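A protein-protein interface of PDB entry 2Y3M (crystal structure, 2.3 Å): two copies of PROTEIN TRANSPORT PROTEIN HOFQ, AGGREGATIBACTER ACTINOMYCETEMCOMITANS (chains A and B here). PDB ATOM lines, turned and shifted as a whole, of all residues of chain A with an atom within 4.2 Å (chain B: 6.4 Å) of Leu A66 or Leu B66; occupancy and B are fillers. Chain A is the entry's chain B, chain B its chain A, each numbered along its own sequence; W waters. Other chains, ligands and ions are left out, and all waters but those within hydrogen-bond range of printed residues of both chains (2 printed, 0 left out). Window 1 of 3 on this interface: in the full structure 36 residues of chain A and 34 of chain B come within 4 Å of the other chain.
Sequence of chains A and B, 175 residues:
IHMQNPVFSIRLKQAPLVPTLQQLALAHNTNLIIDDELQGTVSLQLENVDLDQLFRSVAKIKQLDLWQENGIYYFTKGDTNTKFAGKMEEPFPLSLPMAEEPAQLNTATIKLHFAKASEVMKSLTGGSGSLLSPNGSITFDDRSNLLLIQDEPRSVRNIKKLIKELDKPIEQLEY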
ATOM      1  N   LYS A  13      -7.392  27.160  20.597  1.00  0.00           N
ATOM      2  CA  LYS A  13      -8.276  28.279  20.911  1.00  0.00           C
ATOM      3  C   LYS A  13      -9.680  27.956  20.405  1.00  0.00           C
ATOM      4  O   LYS A  13      -9.826  27.334  19.350  1.00  0.00           O
ATOM      5  CB  LYS A  13      -7.749  29.568  20.264  1.00  0.00           C
ATOM      6  CG  LYS A  13      -8.287  30.857  20.893  1.00  0.00           C
ATOM      7  CD  LYS A  13      -7.814  32.113  20.161  1.00  0.00           C
ATOM      8  CE  LYS A  13      -6.423  32.556  20.621  1.00  0.00           C
ATOM      9  NZ  LYS A  13      -6.103  33.961  20.215  1.00  0.00           N
ATOM     10  N   GLN A  14     -10.706  28.354  21.156  1.00  0.00           N
ATOM     11  CA  GLN A  14     -12.084  28.156  20.705  1.00  0.00           C
ATOM     12  C   GLN A  14     -12.435  29.134  19.595  1.00  0.00           C
ATOM     13  O   GLN A  14     -12.278  30.345  19.749  1.00  0.00           O
ATOM     14  CB  GLN A  14     -13.089  28.261  21.854  1.00  0.00           C
ATOM     15  CG  GLN A  14     -13.530  26.906  22.404  1.00  0.00           C
ATOM     16  CD  GLN A  14     -14.839  26.965  23.173  1.00  0.00           C
ATOM     17  OE1 GLN A  14     -15.266  28.029  23.618  1.00  0.00           O
ATOM     18  NE2 GLN A  14     -15.480  25.812  23.335  1.00  0.00           N
ATOM     19  N   ALA A  15     -12.900  28.588  18.478  1.00  0.00           N
ATOM     20  CA  ALA A  15     -13.249  29.371  17.297  1.00  0.00           C
ATOM     21  C   ALA A  15     -14.459  30.281  17.538  1.00  0.00           C
ATOM     22  O   ALA A  15     -15.310  29.968  18.374  1.00  0.00           O
ATOM     23  CB  ALA A  15     -13.500  28.440  16.116  1.00  0.00           C
ATOM     24  N   LEU A  64     -19.445  20.834  13.314  1.00  0.00           N
ATOM     25  CA  LEU A  64     -18.536  21.983  13.305  1.00  0.00           C
ATOM     26  C   LEU A  64     -17.315  21.749  14.180  1.00  0.00           C
ATOM     27  O   LEU A  64     -17.443  21.364  15.344  1.00  0.00           O
ATOM     28  CB  LEU A  64     -19.242  23.259  13.782  1.00  0.00           C
ATOM     29  CG  LEU A  64     -20.347  23.894  12.934  1.00  0.00           C
ATOM     30  CD1 LEU A  64     -20.958  25.076  13.683  1.00  0.00           C
ATOM     31  CD2 LEU A  64     -19.844  24.323  11.558  1.00  0.00           C
ATOM     32  N   ASP A  65     -16.134  21.982  13.613  1.00  0.00           N
ATOM     33  CA  ASP A  65     -14.906  21.953  14.398  1.00  0.00           C
ATOM     34  C   ASP A  65     -14.786  23.248  15.203  1.00  0.00           C
ATOM     35  O   ASP A  65     -14.675  24.336  14.639  1.00  0.00           O
ATOM     36  CB  ASP A  65     -13.674  21.737  13.511  1.00  0.00           C
ATOM     37  CG  ASP A  65     -12.492  21.157  14.286  1.00  0.00           C
ATOM     38  OD1 ASP A  65     -12.120  21.718  15.341  1.00  0.00           O
ATOM     39  OD2 ASP A  65     -11.936  20.132  13.834  1.00  0.00           O
ATOM     40  N   LEU A  66     -14.804  23.105  16.526  1.00  0.00           N
ATOM     41  CA  LEU A  66     -14.820  24.240  17.447  1.00  0.00           C
ATOM     42  C   LEU A  66     -13.428  24.804  17.777  1.00  0.00           C
ATOM     43  O   LEU A  66     -13.319  25.848  18.424  1.00  0.00           O
ATOM     44  CB  LEU A  66     -15.557  23.856  18.743  1.00  0.00           C
ATOM     45  CG  LEU A  66     -17.034  23.431  18.671  1.00  0.00           C
ATOM     46  CD1 LEU A  66     -17.489  22.881  20.007  1.00  0.00           C
ATOM     47  CD2 LEU A  66     -17.968  24.564  18.218  1.00  0.00           C
ATOM     48  N   TRP A  67     -12.374  24.133  17.321  1.00  0.00           N
ATOM     49  CA  TRP A  67     -11.021  24.478  17.754  1.00  0.00           C
ATOM     50  C   TRP A  67     -10.090  24.887  16.624  1.00  0.00           C
ATOM     51  O   TRP A  67     -10.016  24.223  15.588  1.00  0.00           O
ATOM     52  CB  TRP A  67     -10.412  23.317  18.536  1.00  0.00           C
ATOM     53  CG  TRP A  67     -11.301  22.843  19.637  1.00  0.00           C
ATOM     54  CD1 TRP A  67     -12.227  21.844  19.569  1.00  0.00           C
ATOM     55  CD2 TRP A  67     -11.372  23.369  20.966  1.00  0.00           C
ATOM     56  NE1 TRP A  67     -12.864  21.705  20.775  1.00  0.00           N
ATOM     57  CE2 TRP A  67     -12.359  22.627  21.654  1.00  0.00           C
ATOM     58  CE3 TRP A  67     -10.690  24.389  21.647  1.00  0.00           C
ATOM     59  CZ2 TRP A  67     -12.685  22.872  22.993  1.00  0.00           C
ATOM     60  CZ3 TRP A  67     -11.010  24.630  22.980  1.00  0.00           C
ATOM     61  CH2 TRP A  67     -12.006  23.873  23.639  1.00  0.00           C
ATOM     62  N   LYS B  13     -27.144  22.784  24.634  1.00  0.00           N
ATOM     63  CA  LYS B  13     -26.380  23.379  25.717  1.00  0.00           C
ATOM     64  C   LYS B  13     -24.971  22.820  25.631  1.00  0.00           C
ATOM     65  O   LYS B  13     -24.782  21.601  25.552  1.00  0.00           O
ATOM     66  CB  LYS B  13     -27.035  23.041  27.063  1.00  0.00           C
ATOM     67  CG  LYS B  13     -26.374  23.645  28.303  1.00  0.00           C
ATOM     68  CD  LYS B  13     -27.201  23.319  29.545  1.00  0.00           C
ATOM     69  CE  LYS B  13     -26.357  23.284  30.808  1.00  0.00           C
ATOM     70  NZ  LYS B  13     -26.164  24.636  31.396  1.00  0.00           N
ATOM     71  N   GLN B  14     -23.982  23.708  25.618  1.00  0.00           N
ATOM     72  CA  GLN B  14     -22.601  23.270  25.524  1.00  0.00           C
ATOM     73  C   GLN B  14     -22.173  22.690  26.865  1.00  0.00           C
ATOM     74  O   GLN B  14     -22.358  23.316  27.909  1.00  0.00           O
ATOM     75  CB  GLN B  14     -21.681  24.410  25.086  1.00  0.00           C
ATOM     76  CG  GLN B  14     -20.448  23.918  24.341  1.00  0.00           C
ATOM     77  CD  GLN B  14     -19.454  25.019  24.034  1.00  0.00           C
ATOM     78  OE1 GLN B  14     -18.353  25.048  24.589  1.00  0.00           O
ATOM     79  NE2 GLN B  14     -19.831  25.930  23.144  1.00  0.00           N
ATOM     80  N   ALA B  15     -21.619  21.481  26.816  1.00  0.00           N
ATOM     81  CA  ALA B  15     -21.239  20.724  28.004  1.00  0.00           C
ATOM     82  C   ALA B  15     -20.140  21.420  28.815  1.00  0.00           C
ATOM     83  O   ALA B  15     -19.301  22.120  28.246  1.00  0.00           O
ATOM     84  CB  ALA B  15     -20.807  19.317  27.604  1.00  0.00           C
ATOM     85  N   PRO B  16     -20.155  21.247  30.152  1.00  0.00           N
ATOM     86  CA  PRO B  16     -19.071  21.754  30.991  1.00  0.00           C
ATOM     87  C   PRO B  16     -17.726  21.216  30.508  1.00  0.00           C
ATOM     88  O   PRO B  16     -17.529  19.997  30.424  1.00  0.00           O
ATOM     89  CB  PRO B  16     -19.412  21.197  32.373  1.00  0.00           C
ATOM     90  CG  PRO B  16     -20.884  21.047  32.355  1.00  0.00           C
ATOM     91  CD  PRO B  16     -21.219  20.618  30.958  1.00  0.00           C
ATOM     92  N   LEU B  17     -16.818  22.125  30.178  1.00  0.00           N
ATOM     93  CA  LEU B  17     -15.571  21.757  29.529  1.00  0.00           C
ATOM     94  C   LEU B  17     -14.670  20.880  30.399  1.00  0.00           C
ATOM     95  O   LEU B  17     -14.213  19.823  29.952  1.00  0.00           O
ATOM     96  CB  LEU B  17     -14.831  23.013  29.062  1.00  0.00           C
ATOM     97  CG  LEU B  17     -13.896  22.878  27.860  1.00  0.00           C
ATOM     98  CD1 LEU B  17     -14.506  22.067  26.714  1.00  0.00           C
ATOM     99  CD2 LEU B  17     -13.482  24.256  27.378  1.00  0.00           C
ATOM    100  N   THR B  20     -15.993  17.249  31.004  1.00  0.00           N
ATOM    101  CA  THR B  20     -15.995  16.580  29.702  1.00  0.00           C
ATOM    102  C   THR B  20     -14.585  16.139  29.300  1.00  0.00           C
ATOM    103  O   THR B  20     -14.375  14.990  28.901  1.00  0.00           O
ATOM    104  CB  THR B  20     -16.572  17.496  28.588  1.00  0.00           C
ATOM    105  OG1 THR B  20     -17.911  17.890  28.918  1.00  0.00           O
ATOM    106  CG2 THR B  20     -16.578  16.782  27.245  1.00  0.00           C
ATOM    107  N   LEU B  21     -13.626  17.058  29.409  1.00  0.00           N
ATOM    108  CA  LEU B  21     -12.244  16.787  29.020  1.00  0.00           C
ATOM    109  C   LEU B  21     -11.584  15.761  29.935  1.00  0.00           C
ATOM    110  O   LEU B  21     -10.783  14.941  29.483  1.00  0.00           O
ATOM    111  CB  LEU B  21     -11.429  18.081  29.006  1.00  0.00           C
ATOM    112  CG  LEU B  21     -11.669  19.051  27.850  1.00  0.00           C
ATOM    113  CD1 LEU B  21     -11.008  20.389  28.139  1.00  0.00           C
ATOM    114  CD2 LEU B  21     -11.165  18.467  26.537  1.00  0.00           C
ATOM    115  N   ILE B  61      -9.900  15.798  21.038  1.00  0.00           N
ATOM    116  CA  ILE B  61     -10.620  17.003  21.448  1.00  0.00           C
ATOM    117  C   ILE B  61     -11.493  17.545  20.304  1.00  0.00           C
ATOM    118  O   ILE B  61     -12.632  17.960  20.525  1.00  0.00           O
ATOM    119  CB  ILE B  61      -9.657  18.084  21.996  1.00  0.00           C
ATOM    120  CG1 ILE B  61      -9.026  17.594  23.308  1.00  0.00           C
ATOM    121  CG2 ILE B  61     -10.388  19.411  22.213  1.00  0.00           C
ATOM    122  CD1 ILE B  61      -7.787  18.341  23.727  1.00  0.00           C
ATOM    123  N   LYS B  62     -10.965  17.513  19.085  1.00  0.00           N
ATOM    124  CA  LYS B  62     -11.702  17.994  17.921  1.00  0.00           C
ATOM    125  C   LYS B  62     -12.913  17.123  17.583  1.00  0.00           C
ATOM    126  O   LYS B  62     -13.964  17.645  17.208  1.00  0.00           O
ATOM    127  CB  LYS B  62     -10.780  18.111  16.709  1.00  0.00           C
ATOM    128  CG  LYS B  62      -9.780  19.236  16.813  1.00  0.00           C
ATOM    129  CD  LYS B  62      -9.008  19.368  15.522  1.00  0.00           C
ATOM    130  CE  LYS B  62      -8.218  20.652  15.499  1.00  0.00           C
ATOM    131  NZ  LYS B  62      -7.470  20.796  14.220  1.00  0.00           N
ATOM    132  N   LEU B  64     -14.614  15.618  19.635  1.00  0.00           N
ATOM    133  CA  LEU B  64     -15.467  15.663  20.811  1.00  0.00           C
ATOM    134  C   LEU B  64     -16.745  16.441  20.539  1.00  0.00           C
ATOM    135  O   LEU B  64     -16.696  17.599  20.120  1.00  0.00           O
ATOM    136  CB  LEU B  64     -14.695  16.283  21.979  1.00  0.00           C
ATOM    137  CG  LEU B  64     -15.292  16.395  23.382  1.00  0.00           C
ATOM    138  CD1 LEU B  64     -15.631  15.030  23.967  1.00  0.00           C
ATOM    139  CD2 LEU B  64     -14.308  17.139  24.268  1.00  0.00           C
ATOM    140  N   ASP B  65     -17.885  15.793  20.767  1.00  0.00           N
ATOM    141  CA  ASP B  65     -19.184  16.438  20.612  1.00  0.00           C
ATOM    142  C   ASP B  65     -19.598  17.056  21.944  1.00  0.00           C
ATOM    143  O   ASP B  65     -19.968  16.347  22.883  1.00  0.00           O
ATOM    144  CB  ASP B  65     -20.234  15.441  20.106  1.00  0.00           C
ATOM    145  CG  ASP B  65     -21.572  16.102  19.773  1.00  0.00           C
ATOM    146  OD1 ASP B  65     -21.705  17.338  19.919  1.00  0.00           O
ATOM    147  OD2 ASP B  65     -22.502  15.375  19.359  1.00  0.00           O
ATOM    148  N   LEU B  66     -19.528  18.382  22.009  1.00  0.00           N
ATOM    149  CA  LEU B  66     -19.764  19.127  23.243  1.00  0.00           C
ATOM    150  C   LEU B  66     -21.224  19.519  23.463  1.00  0.00           C
ATOM    151  O   LEU B  66     -21.564  20.085  24.501  1.00  0.00           O
ATOM    152  CB  LEU B  66     -18.906  20.397  23.263  1.00  0.00           C
ATOM    153  CG  LEU B  66     -17.391  20.272  23.422  1.00  0.00           C
ATOM    154  CD1 LEU B  66     -16.726  21.584  23.058  1.00  0.00           C
ATOM    155  CD2 LEU B  66     -17.005  19.837  24.841  1.00  0.00           C
ATOM    156  N   TRP B  67     -22.086  19.229  22.496  1.00  0.00           N
ATOM    157  CA  TRP B  67     -23.468  19.699  22.560  1.00  0.00           C
ATOM    158  C   TRP B  67     -24.434  18.676  23.159  1.00  0.00           C
ATOM    159  O   TRP B  67     -24.651  17.601  22.592  1.00  0.00           O
ATOM    160  CB  TRP B  67     -23.951  20.152  21.174  1.00  0.00           C
ATOM    161  CG  TRP B  67     -23.092  21.223  20.552  1.00  0.00           C
ATOM    162  CD1 TRP B  67     -22.121  21.049  19.609  1.00  0.00           C
ATOM    163  CD2 TRP B  67     -23.125  22.629  20.838  1.00  0.00           C
ATOM    164  NE1 TRP B  67     -21.547  22.256  19.288  1.00  0.00           N
ATOM    165  CE2 TRP B  67     -22.143  23.243  20.029  1.00  0.00           C
ATOM    166  CE3 TRP B  67     -23.887  23.428  21.703  1.00  0.00           C
ATOM    167  CZ2 TRP B  67     -21.904  24.623  20.054  1.00  0.00           C
ATOM    168  CZ3 TRP B  67     -23.653  24.792  21.729  1.00  0.00           C
ATOM    169  CH2 TRP B  67     -22.667  25.379  20.909  1.00  0.00           C
ATOM    170  N   GLN B  68     -25.011  19.026  24.306  1.00  0.00           N
ATOM    171  CA  GLN B  68     -26.067  18.231  24.935  1.00  0.00           C
ATOM    172  C   GLN B  68     -27.454  18.628  24.407  1.00  0.00           C
ATOM    173  O   GLN B  68     -27.812  19.809  24.430  1.00  0.00           O
ATOM    174  CB  GLN B  68     -26.018  18.400  26.454  1.00  0.00           C
ATOM    175  CG  GLN B  68     -24.710  17.936  27.094  1.00  0.00           C
ATOM    176  CD  GLN B  68     -24.528  18.439  28.519  1.00  0.00           C
ATOM    177  OE1 GLN B  68     -25.195  19.381  28.956  1.00  0.00           O
ATOM    178  NE2 GLN B  68     -23.610  17.816  29.247  1.00  0.00           N
HETATM  179  O   HOH W   1     -19.274  21.303  17.131  1.00  0.00           O
HETATM  180  O   HOH W   2     -14.876  19.456  20.212  1.00  0.00           O
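The side-chain amide nitrogen (NE2) of Gln A14 is in hydrogen-bond range of the side-chain amide oxygen (OE1) of Gln B14 (3.2 Å).
N of Ala B15 sits at hydrogen-bond distance from O of Leu B66 (2.7 Å). The backbone NH of Ala A15 sits at hydrogen-bond distance from the backbone carbonyl oxygen of Leu A66 (2.8 Å). The side-chain carboxylate of Asp A65 is in hydrogen-bond range of the backbone NH of Trp A67 (3.1 Å).
Among the printed residues, merely in contact across the chains: Asp A65 with Lys B62, Leu A66 with Leu B66, Trp A67 with Ile B61 and Trp A67 with Lys B62.
Leu B66 touches one residue of chain A. Printed residues of chain A within 4 Å of Ile B61: Trp A67. Of the printed residues of chain A, Gln B14 touches Gln A14. Printed residues of chain B within 4 Å of Asp A65: Lys B62 (3.5 Å). Of the printed residues of chain A, Lys B62 touches Asp A65 (3.5 Å) and Trp A67 (3.999 Å). Of the printed residues of chain B, Gln A14 touches Gln B14. Thr B20 touches none of the printed residues of chain A. Ala A15 touches none of the printed residues of chain B. The nearest residue of chain B that does not touch Leu A66 is Trp B67 (4.2 Å). The nearest printed residue of chain A that does not touch Leu B66 is Trp A67 (4.2 Å).
Of the 7 printed residues of chain A, 4 touch a printed residue of chain B. Printed residues of chain A that touch a printed residue of chain B: Gln A14, Asp A65, Leu A66 and Trp A67. Hydrophobic or aromatic side chains of chain A that line the printed part of chain B: Leu A66 and Trp A67. Of the 14 printed residues of chain B, 4 touch a printed residue of chain A. Hydrophobic or aromatic side chains of chain B within 4 Å of the printed part of chain A: Ile B61 and Leu B66. Along chain B the printed residues that touch a printed residue of chain A span positions 14 to 66. Among the printed residues, 5 pairs touch across the chains.
Gln B14 touches its own counterpart, Gln A14. Leu A66 touches its own counterpart, Leu B66. Positions printed for both chains: 13, 14, 15, 64, 65, 66 and 67. Of the 5 pairs that touch across the chains among the printed residues, 2 have their exchanged pair printed and touching as well.
Water W1 lies within hydrogen-bond range of O of Leu A64 (2.6 Å) and NE1 of Trp B67 (3.3 Å). Water W2 lies within hydrogen-bond range of the backbone carbonyl oxygen of Leu B64 (2.6 Å), the backbone carbonyl oxygen of Ile B61 (2.7 Å) and the indole nitrogen of Trp A67 (3.1 Å).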
